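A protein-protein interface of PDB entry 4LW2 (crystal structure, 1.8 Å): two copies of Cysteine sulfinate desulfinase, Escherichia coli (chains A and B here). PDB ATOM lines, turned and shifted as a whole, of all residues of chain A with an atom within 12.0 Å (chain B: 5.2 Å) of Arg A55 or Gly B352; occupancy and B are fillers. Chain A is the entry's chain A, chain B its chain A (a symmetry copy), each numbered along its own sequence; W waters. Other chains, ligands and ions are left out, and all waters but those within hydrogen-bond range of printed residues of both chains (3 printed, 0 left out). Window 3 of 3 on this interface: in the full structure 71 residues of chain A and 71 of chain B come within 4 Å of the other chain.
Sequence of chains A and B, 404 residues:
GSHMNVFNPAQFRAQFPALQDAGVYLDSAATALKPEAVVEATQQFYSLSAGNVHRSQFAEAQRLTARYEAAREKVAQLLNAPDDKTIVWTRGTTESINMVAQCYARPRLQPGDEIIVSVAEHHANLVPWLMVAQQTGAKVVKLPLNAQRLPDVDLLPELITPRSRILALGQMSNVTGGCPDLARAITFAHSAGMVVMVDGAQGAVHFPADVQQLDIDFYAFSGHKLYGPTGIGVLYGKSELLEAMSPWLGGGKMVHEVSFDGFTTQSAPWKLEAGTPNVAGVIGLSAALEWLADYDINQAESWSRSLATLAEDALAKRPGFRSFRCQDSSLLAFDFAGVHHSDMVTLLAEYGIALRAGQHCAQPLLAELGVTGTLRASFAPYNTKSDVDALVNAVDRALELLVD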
ATOM      1  N   GLN A  44     -37.617 -10.264   6.720  1.00  0.00           N
ATOM      2  CA  GLN A  44     -36.552 -10.106   7.736  1.00  0.00           C
ATOM      3  C   GLN A  44     -37.204  -9.971   9.116  1.00  0.00           C
ATOM      4  O   GLN A  44     -36.750 -10.616  10.065  1.00  0.00           O
ATOM      5  CB  GLN A  44     -35.680  -8.909   7.416  1.00  0.00           C
ATOM      6  CG  GLN A  44     -34.825  -9.295   6.198  1.00  0.00           C
ATOM      7  CD  GLN A  44     -33.957 -10.487   6.454  1.00  0.00           C
ATOM      8  OE1 GLN A  44     -33.644 -10.789   7.621  1.00  0.00           O
ATOM      9  NE2 GLN A  44     -33.599 -11.215   5.403  1.00  0.00           N
ATOM     10  N   SER A  47     -38.122 -13.300  10.398  1.00  0.00           N
ATOM     11  CA  SER A  47     -37.043 -14.323  10.289  1.00  0.00           C
ATOM     12  C   SER A  47     -35.941 -14.033  11.331  1.00  0.00           C
ATOM     13  O   SER A  47     -34.961 -14.792  11.428  1.00  0.00           O
ATOM     14  CB  SER A  47     -36.414 -14.259   8.829  1.00  0.00           C
ATOM     15  OG  SER A  47     -37.373 -14.936   8.029  1.00  0.00           O
ATOM     16  N   LEU A  48     -36.115 -12.958  12.098  1.00  0.00           N
ATOM     17  CA  LEU A  48     -35.127 -12.507  13.118  1.00  0.00           C
ATOM     18  C   LEU A  48     -35.814 -12.253  14.453  1.00  0.00           C
ATOM     19  O   LEU A  48     -36.970 -11.700  14.547  1.00  0.00           O
ATOM     20  CB  LEU A  48     -34.454 -11.183  12.653  1.00  0.00           C
ATOM     21  CG  LEU A  48     -33.597 -11.297  11.376  1.00  0.00           C
ATOM     22  CD1 LEU A  48     -33.116  -9.882  10.844  1.00  0.00           C
ATOM     23  CD2 LEU A  48     -32.443 -12.281  11.497  1.00  0.00           C
ATOM     24  N   SER A  49     -35.038 -12.454  15.526  1.00  0.00           N
ATOM     25  CA  SER A  49     -35.488 -12.079  16.831  1.00  0.00           C
ATOM     26  C   SER A  49     -35.755 -10.570  16.947  1.00  0.00           C
ATOM     27  O   SER A  49     -34.994  -9.797  16.404  1.00  0.00           O
ATOM     28  CB  SER A  49     -34.357 -12.448  17.817  1.00  0.00           C
ATOM     29  OG  SER A  49     -34.712 -12.004  19.126  1.00  0.00           O
ATOM     30  N   ALA A  50     -36.781 -10.164  17.685  1.00  0.00           N
ATOM     31  CA  ALA A  50     -36.972  -8.708  17.951  1.00  0.00           C
ATOM     32  C   ALA A  50     -36.287  -8.342  19.264  1.00  0.00           C
ATOM     33  O   ALA A  50     -36.382  -7.179  19.742  1.00  0.00           O
ATOM     34  CB  ALA A  50     -38.507  -8.322  18.035  1.00  0.00           C
ATOM     35  N   GLY A  51     -35.636  -9.342  19.870  1.00  0.00           N
ATOM     36  CA  GLY A  51     -34.898  -9.114  21.115  1.00  0.00           C
ATOM     37  C   GLY A  51     -33.590  -8.356  21.004  1.00  0.00           C
ATOM     38  O   GLY A  51     -33.196  -7.885  19.914  1.00  0.00           O
ATOM     39  N   ASN A  52     -32.865  -8.359  22.129  1.00  0.00           N
ATOM     40  CA  ASN A  52     -31.626  -7.551  22.262  1.00  0.00           C
ATOM     41  C   ASN A  52     -30.318  -8.259  21.848  1.00  0.00           C
ATOM     42  O   ASN A  52     -29.206  -7.702  22.046  1.00  0.00           O
ATOM     43  CB  ASN A  52     -31.523  -6.901  23.680  1.00  0.00           C
ATOM     44  CG  ASN A  52     -31.632  -7.948  24.899  1.00  0.00           C
ATOM     45  OD1 ASN A  52     -31.782  -7.561  26.082  1.00  0.00           O
ATOM     46  ND2 ASN A  52     -31.549  -9.241  24.588  1.00  0.00           N
ATOM     47  N   VAL A  53     -30.435  -9.502  21.380  1.00  0.00           N
ATOM     48  CA  VAL A  53     -29.291 -10.287  20.931  1.00  0.00           C
ATOM     49  C   VAL A  53     -29.304 -10.614  19.420  1.00  0.00           C
ATOM     50  O   VAL A  53     -30.313 -11.091  18.871  1.00  0.00           O
ATOM     51  CB  VAL A  53     -29.189 -11.607  21.779  1.00  0.00           C
ATOM     52  CG1 VAL A  53     -28.084 -12.557  21.212  1.00  0.00           C
ATOM     53  CG2 VAL A  53     -28.897 -11.248  23.306  1.00  0.00           C
ATOM     54  N   HIS A  54     -28.171 -10.376  18.751  1.00  0.00           N
ATOM     55  CA  HIS A  54     -28.005 -10.782  17.400  1.00  0.00           C
ATOM     56  C   HIS A  54     -26.663 -11.355  17.130  1.00  0.00           C
ATOM     57  O   HIS A  54     -25.739 -10.614  16.951  1.00  0.00           O
ATOM     58  CB  HIS A  54     -28.305  -9.580  16.441  1.00  0.00           C
ATOM     59  CG  HIS A  54     -29.732  -9.122  16.552  1.00  0.00           C
ATOM     60  ND1 HIS A  54     -30.788  -9.873  16.066  1.00  0.00           N
ATOM     61  CD2 HIS A  54     -30.278  -8.080  17.217  1.00  0.00           C
ATOM     62  CE1 HIS A  54     -31.925  -9.303  16.418  1.00  0.00           C
ATOM     63  NE2 HIS A  54     -31.643  -8.192  17.085  1.00  0.00           N
ATOM     64  N   ARG A  55     -26.559 -12.670  16.992  1.00  0.00           N
ATOM     65  CA  ARG A  55     -25.239 -13.260  16.911  1.00  0.00           C
ATOM     66  C   ARG A  55     -24.661 -13.244  15.508  1.00  0.00           C
ATOM     67  O   ARG A  55     -23.432 -13.369  15.318  1.00  0.00           O
ATOM     68  CB  ARG A  55     -25.290 -14.699  17.432  1.00  0.00           C
ATOM     69  CG  ARG A  55     -26.010 -14.896  18.807  1.00  0.00           C
ATOM     70  CD  ARG A  55     -25.362 -14.167  19.933  1.00  0.00           C
ATOM     71  NE  ARG A  55     -24.263 -14.950  20.505  1.00  0.00           N
ATOM     72  CZ  ARG A  55     -23.388 -14.464  21.392  1.00  0.00           C
ATOM     73  NH1 ARG A  55     -22.419 -15.255  21.835  1.00  0.00           N
ATOM     74  NH2 ARG A  55     -23.505 -13.223  21.848  1.00  0.00           N
ATOM     75  N   SER A  56     -25.521 -13.107  14.494  1.00  0.00           N
ATOM     76  CA  SER A  56     -25.027 -13.105  13.098  1.00  0.00           C
ATOM     77  C   SER A  56     -25.684 -12.049  12.165  1.00  0.00           C
ATOM     78  O   SER A  56     -25.056 -11.663  11.189  1.00  0.00           O
ATOM     79  CB  SER A  56     -25.210 -14.493  12.494  1.00  0.00           C
ATOM     80  OG  SER A  56     -26.578 -14.871  12.601  1.00  0.00           O
ATOM     81  N   GLN A  57     -26.908 -11.558  12.438  1.00  0.00           N
ATOM     82  CA  GLN A  57     -27.541 -10.636  11.483  1.00  0.00           C
ATOM     83  C   GLN A  57     -27.760  -9.283  12.147  1.00  0.00           C
ATOM     84  O   GLN A  57     -28.851  -8.720  12.045  1.00  0.00           O
ATOM     85  CB  GLN A  57     -28.902 -11.175  11.004  1.00  0.00           C
ATOM     86  CG  GLN A  57     -28.863 -12.619  10.498  1.00  0.00           C
ATOM     87  CD  GLN A  57     -27.999 -12.692   9.257  1.00  0.00           C
ATOM     88  OE1 GLN A  57     -27.012 -13.426   9.211  1.00  0.00           O
ATOM     89  NE2 GLN A  57     -28.324 -11.885   8.277  1.00  0.00           N
ATOM     90  N   PHE A  58     -26.737  -8.758  12.798  1.00  0.00           N
ATOM     91  CA  PHE A  58     -26.898  -7.515  13.505  1.00  0.00           C
ATOM     92  C   PHE A  58     -27.265  -6.396  12.484  1.00  0.00           C
ATOM     93  O   PHE A  58     -28.056  -5.524  12.790  1.00  0.00           O
ATOM     94  CB  PHE A  58     -25.623  -7.150  14.232  1.00  0.00           C
ATOM     95  CG  PHE A  58     -25.739  -5.880  15.044  1.00  0.00           C
ATOM     96  CD1 PHE A  58     -26.863  -5.659  15.916  1.00  0.00           C
ATOM     97  CD2 PHE A  58     -24.785  -4.893  14.927  1.00  0.00           C
ATOM     98  CE1 PHE A  58     -26.982  -4.474  16.667  1.00  0.00           C
ATOM     99  CE2 PHE A  58     -24.879  -3.704  15.662  1.00  0.00           C
ATOM    100  CZ  PHE A  58     -25.961  -3.488  16.534  1.00  0.00           C
ATOM    101  N   ALA A  59     -26.617  -6.412  11.319  1.00  0.00           N
ATOM    102  CA  ALA A  59     -26.886  -5.368  10.283  1.00  0.00           C
ATOM    103  C   ALA A  59     -28.379  -5.287   9.915  1.00  0.00           C
ATOM    104  O   ALA A  59     -28.967  -4.189   9.863  1.00  0.00           O
ATOM    105  CB  ALA A  59     -26.057  -5.648   9.050  1.00  0.00           C
ATOM    106  N   GLU A  60     -28.958  -6.458   9.628  1.00  0.00           N
ATOM    107  CA  GLU A  60     -30.394  -6.565   9.224  1.00  0.00           C
ATOM    108  C   GLU A  60     -31.270  -6.105  10.383  1.00  0.00           C
ATOM    109  O   GLU A  60     -32.289  -5.407  10.170  1.00  0.00           O
ATOM    110  CB  GLU A  60     -30.741  -8.010   8.856  1.00  0.00           C
ATOM    111  CG  GLU A  60     -29.995  -8.473   7.571  1.00  0.00           C
ATOM    112  CD  GLU A  60     -30.441  -9.865   7.029  1.00  0.00           C
ATOM    113  OE1 GLU A  60     -31.100 -10.675   7.794  1.00  0.00           O
ATOM    114  OE2 GLU A  60     -30.115 -10.145   5.817  1.00  0.00           O
ATOM    115  N   ALA A  61     -30.891  -6.507  11.601  1.00  0.00           N
ATOM    116  CA  ALA A  61     -31.668  -6.086  12.772  1.00  0.00           C
ATOM    117  C   ALA A  61     -31.612  -4.578  13.018  1.00  0.00           C
ATOM    118  O   ALA A  61     -32.601  -3.947  13.322  1.00  0.00           O
ATOM    119  CB  ALA A  61     -31.241  -6.870  13.995  1.00  0.00           C
ATOM    120  N   GLN A  62     -30.456  -3.974  12.806  1.00  0.00           N
ATOM    121  CA  GLN A  62     -30.391  -2.529  12.979  1.00  0.00           C
ATOM    122  C   GLN A  62     -31.208  -1.751  11.912  1.00  0.00           C
ATOM    123  O   GLN A  62     -31.810  -0.693  12.205  1.00  0.00           O
ATOM    124  CB  GLN A  62     -28.880  -2.163  12.976  1.00  0.00           C
ATOM    125  CG  GLN A  62     -28.516  -0.752  12.964  1.00  0.00           C
ATOM    126  CD  GLN A  62     -26.934  -0.682  13.023  1.00  0.00           C
ATOM    127  OE1 GLN A  62     -26.381   0.250  13.628  1.00  0.00           O
ATOM    128  NE2 GLN A  62     -26.225  -1.702  12.405  1.00  0.00           N
ATOM    129  N   GLN B  20     -30.640 -19.348  15.287  1.00  0.00           N
ATOM    130  CA  GLN B  20     -29.228 -19.143  15.231  1.00  0.00           C
ATOM    131  C   GLN B  20     -28.791 -17.652  15.622  1.00  0.00           C
ATOM    132  O   GLN B  20     -28.021 -17.429  16.611  1.00  0.00           O
ATOM    133  CB  GLN B  20     -28.764 -19.695  13.867  1.00  0.00           C
ATOM    134  CG  GLN B  20     -29.489 -20.883  13.226  1.00  0.00           C
ATOM    135  CD  GLN B  20     -30.963 -20.631  12.930  1.00  0.00           C
ATOM    136  OE1 GLN B  20     -31.311 -19.677  12.227  1.00  0.00           O
ATOM    137  NE2 GLN B  20     -31.838 -21.503  13.460  1.00  0.00           N
ATOM    138  N   ASP B  21     -29.337 -16.650  14.922  1.00  0.00           N
ATOM    139  CA  ASP B  21     -29.020 -15.280  15.257  1.00  0.00           C
ATOM    140  C   ASP B  21     -29.531 -14.869  16.662  1.00  0.00           C
ATOM    141  O   ASP B  21     -28.979 -13.936  17.277  1.00  0.00           O
ATOM    142  CB  ASP B  21     -29.688 -14.348  14.206  1.00  0.00           C
ATOM    143  CG  ASP B  21     -29.497 -12.901  14.514  1.00  0.00           C
ATOM    144  OD1 ASP B  21     -28.325 -12.398  14.465  1.00  0.00           O
ATOM    145  OD2 ASP B  21     -30.507 -12.267  14.908  1.00  0.00           O
ATOM    146  N   ALA B  22     -30.610 -15.510  17.119  1.00  0.00           N
ATOM    147  CA  ALA B  22     -31.291 -14.984  18.340  1.00  0.00           C
ATOM    148  C   ALA B  22     -30.467 -15.212  19.635  1.00  0.00           C
ATOM    149  O   ALA B  22     -30.831 -14.597  20.706  1.00  0.00           O
ATOM    150  CB  ALA B  22     -32.615 -15.687  18.531  1.00  0.00           C
ATOM    151  N   GLY B  23     -29.545 -16.195  19.573  1.00  0.00           N
ATOM    152  CA  GLY B  23     -28.725 -16.563  20.785  1.00  0.00           C
ATOM    153  C   GLY B  23     -29.659 -17.407  21.626  1.00  0.00           C
ATOM    154  O   GLY B  23     -30.297 -18.330  21.116  1.00  0.00           O
ATOM    155  N   VAL B  24     -29.700 -17.096  22.903  1.00  0.00           N
ATOM    156  CA  VAL B  24     -30.533 -17.846  23.853  1.00  0.00           C
ATOM    157  C   VAL B  24     -31.730 -16.930  24.090  1.00  0.00           C
ATOM    158  O   VAL B  24     -31.595 -15.929  24.800  1.00  0.00           O
ATOM    159  CB  VAL B  24     -29.715 -18.022  25.148  1.00  0.00           C
ATOM    160  CG1 VAL B  24     -30.584 -18.528  26.263  1.00  0.00           C
ATOM    161  CG2 VAL B  24     -28.480 -18.979  24.891  1.00  0.00           C
ATOM    162  N   LEU B 348     -26.509  -9.561  30.460  1.00  0.00           N
ATOM    163  CA  LEU B 348     -26.956 -10.851  29.900  1.00  0.00           C
ATOM    164  C   LEU B 348     -26.956 -10.841  28.370  1.00  0.00           C
ATOM    165  O   LEU B 348     -26.528 -11.794  27.727  1.00  0.00           O
ATOM    166  CB  LEU B 348     -28.286 -11.319  30.475  1.00  0.00           C
ATOM    167  CG  LEU B 348     -28.392 -11.588  31.966  1.00  0.00           C
ATOM    168  CD1 LEU B 348     -29.769 -12.156  32.416  1.00  0.00           C
ATOM    169  CD2 LEU B 348     -27.253 -12.336  32.578  1.00  0.00           C
ATOM    170  N   ALA B 349     -27.335  -9.718  27.803  1.00  0.00           N
ATOM    171  CA  ALA B 349     -27.387  -9.597  26.351  1.00  0.00           C
ATOM    172  C   ALA B 349     -25.983  -9.697  25.729  1.00  0.00           C
ATOM    173  O   ALA B 349     -25.793 -10.313  24.679  1.00  0.00           O
ATOM    174  CB  ALA B 349     -28.102  -8.233  25.941  1.00  0.00           C
ATOM    175  N   GLU B 350     -24.981  -9.217  26.464  1.00  0.00           N
ATOM    176  CA  GLU B 350     -23.568  -9.374  26.000  1.00  0.00           C
ATOM    177  C   GLU B 350     -23.146 -10.794  26.035  1.00  0.00           C
ATOM    178  O   GLU B 350     -22.317 -11.233  25.224  1.00  0.00           O
ATOM    179  CB  GLU B 350     -22.561  -8.599  26.922  1.00  0.00           C
ATOM    180  CG  GLU B 350     -22.823  -7.176  27.082  1.00  0.00           C
ATOM    181  CD  GLU B 350     -22.420  -6.315  25.896  1.00  0.00           C
ATOM    182  OE1 GLU B 350     -22.532  -6.704  24.709  1.00  0.00           O
ATOM    183  OE2 GLU B 350     -22.000  -5.183  26.168  1.00  0.00           O
ATOM    184  N   TYR B 351     -23.759 -11.557  26.933  1.00  0.00           N
ATOM    185  CA  TYR B 351     -23.548 -13.012  26.928  1.00  0.00           C
ATOM    186  C   TYR B 351     -24.442 -13.721  25.936  1.00  0.00           C
ATOM    187  O   TYR B 351     -24.341 -14.982  25.847  1.00  0.00           O
ATOM    188  CB  TYR B 351     -23.793 -13.591  28.354  1.00  0.00           C
ATOM    189  CG  TYR B 351     -22.563 -13.457  29.226  1.00  0.00           C
ATOM    190  CD1 TYR B 351     -22.148 -12.205  29.654  1.00  0.00           C
ATOM    191  CD2 TYR B 351     -21.775 -14.601  29.535  1.00  0.00           C
ATOM    192  CE1 TYR B 351     -20.964 -12.072  30.426  1.00  0.00           C
ATOM    193  CE2 TYR B 351     -20.591 -14.493  30.252  1.00  0.00           C
ATOM    194  CZ  TYR B 351     -20.201 -13.253  30.696  1.00  0.00           C
ATOM    195  OH  TYR B 351     -19.024 -13.143  31.399  1.00  0.00           O
ATOM    196  N   GLY B 352     -25.213 -12.992  25.104  1.00  0.00           N
ATOM    197  CA  GLY B 352     -26.070 -13.678  24.129  1.00  0.00           C
ATOM    198  C   GLY B 352     -27.391 -14.192  24.694  1.00  0.00           C
ATOM    199  O   GLY B 352     -28.062 -15.077  24.065  1.00  0.00           O
ATOM    200  N   ILE B 353     -27.796 -13.629  25.834  1.00  0.00           N
ATOM    201  CA  ILE B 353     -29.047 -14.115  26.512  1.00  0.00           C
ATOM    202  C   ILE B 353     -30.078 -12.934  26.333  1.00  0.00           C
ATOM    203  O   ILE B 353     -29.798 -11.803  26.851  1.00  0.00           O
ATOM    204  CB  ILE B 353     -28.823 -14.349  27.984  1.00  0.00           C
ATOM    205  CG1 ILE B 353     -27.602 -15.265  28.314  1.00  0.00           C
ATOM    206  CG2 ILE B 353     -30.114 -14.881  28.632  1.00  0.00           C
ATOM    207  CD1 ILE B 353     -27.715 -16.635  27.737  1.00  0.00           C
ATOM    208  N   ALA B 354     -31.231 -13.207  25.668  1.00  0.00           N
ATOM    209  CA  ALA B 354     -32.229 -12.158  25.441  1.00  0.00           C
ATOM    210  C   ALA B 354     -33.353 -12.337  26.444  1.00  0.00           C
ATOM    211  O   ALA B 354     -34.170 -13.318  26.352  1.00  0.00           O
ATOM    212  CB  ALA B 354     -32.833 -12.241  23.996  1.00  0.00           C
HETATM  213  O   HOH W   1     -30.929  -9.586  27.969  1.00  0.00           O
HETATM  214  O   HOH W   2     -32.353 -12.207  20.393  1.00  0.00           O
HETATM  215  O   HOH W   3     -32.683 -13.711  15.220  1.00  0.00           O
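Water W3 lies within hydrogen-bond range of OD2 of Asp B21 (2.6 Å), N of Ser A49 (2.7 Å) and N of Ala B22 (3.3 Å). Water W2 lies within hydrogen-bond range of the side-chain hydroxyl of Ser A49 (2.7 Å), the backbone carbonyl oxygen of Val A53 (2.8 Å) and the backbone carbonyl oxygen of Ala B22 (2.9 Å). Water W1 bridges the backbone carbonyl oxygen of Ile B353 (2.7 Å) and the side-chain amide oxygen of Asn A52 (2.9 Å).
Of the 12 printed residues of chain B, 8 touch a printed residue of chain A. Hydrophobic or aromatic side chains of chain A that line the printed part of chain B: Leu A48, Val A53 and His A54. Among the printed residues, 18 pairs touch across the chains. Among the printed residues, no Asp or Glu carboxylate lies within 4 Å of a Lys or Arg side-chain nitrogen of the other chain.
OG of Ser A49 sits at hydrogen-bond distance from N of Gly A51, 2.9 Å away. NE2 of His A54 lies within hydrogen-bond range of O of Gly A51, 3.2 Å away. The side-chain amide nitrogen (NE2) of Gln A57 is in hydrogen-bond range of the side-chain carboxylate (OE1) of Glu A60, 3.1 Å away. O of Gly B352 lies within hydrogen-bond range of N of Val B24 (2.8 Å). The backbone carbonyl oxygen (O) of Val B24 sits at hydrogen-bond distance from the backbone NH (N) of Ala B354 (2.9 Å). The backbone carbonyl oxygen (O) of Leu B348 lies within hydrogen-bond range of the backbone NH (N) of Ile B353 (2.9 Å).
ND1 of His A54 is in hydrogen-bond range of OD2 of Asp B21 (2.7 Å). N of Arg A55 sits at hydrogen-bond distance from O of Asp B21, 2.7 Å away. The backbone NH (N) of Ser A56 sits at hydrogen-bond distance from the side-chain carboxylate (OD1) of Asp B21 (2.9 Å). N of Gln A57 lies within hydrogen-bond range of OD1 of Asp B21, at 2.6 Å.
Of the printed residues of chain B, Leu A48 touches Asp B21. Of the printed residues of chain B, Asn A52 touches Ala B349 (3.7 Å), Ile B353 (3.8 Å) and Ala B354 (3.1 Å). Printed residues of chain B within 4 Å of Val A53: Asp B21 (3.5 Å), Ala B22 (3.5 Å), Ala B349 (3.5 Å), Gly B352 (3.6 Å), Ile B353 (3.6 Å) and Ala B354 (3.9 Å). Of chain B, only Gln B20 (3.9 Å), Asp B21 (2.7 Å), Gly B23 (3.8 Å) and Gly B352 (3.5 Å) come within 4 Å of Arg A55. Of the printed residues of chain B, Ser A56 touches Asp B21. Of the printed residues of chain B, Gln A57 touches Asp B21. Of chain A, only Leu A48, Val A53, His A54, Arg A55, Ser A56 and Gln A57 come within 4 Å of Asp B21. Of chain A, only Arg A55 comes within 4 Å of Gly B23. Gly B352 touches two residues of chain A. Of the printed residues of chain A, Ala B354 touches Asn A52 and Val A53. The nearest residue of chain B that does not touch Arg A55 is Glu B350 (4.1 Å). The nearest residue of chain A that does not touch Gly B352 is Asn A52 (6.5 Å).
No position is printed for both chains.
Among the printed residues, pairs that only touch across the chains: Asn A52 with Ala B354 (3.1 Å), Val A53 with Ala B22 (3.5 Å), Arg A55 with Gly B352 (3.5 Å), Val A53 with Ala B349 (3.5 Å), Val A53 with Asp B21 (3.5 Å), Val A53 with Gly B352 (3.6 Å), Val A53 with Ile B353 (3.6 Å), Asn A52 with Ala B349 (3.7 Å), Ser A49 with Ala B22 (3.7 Å), Arg A55 with Gly B23 (3.8 Å), Asn A52 with Ile B353 (3.8 Å), Val A53 with Ala B354 (3.9 Å), Arg A55 with Gln B20 (3.9 Å) and Leu A48 with Asp B21 (3.9 Å).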
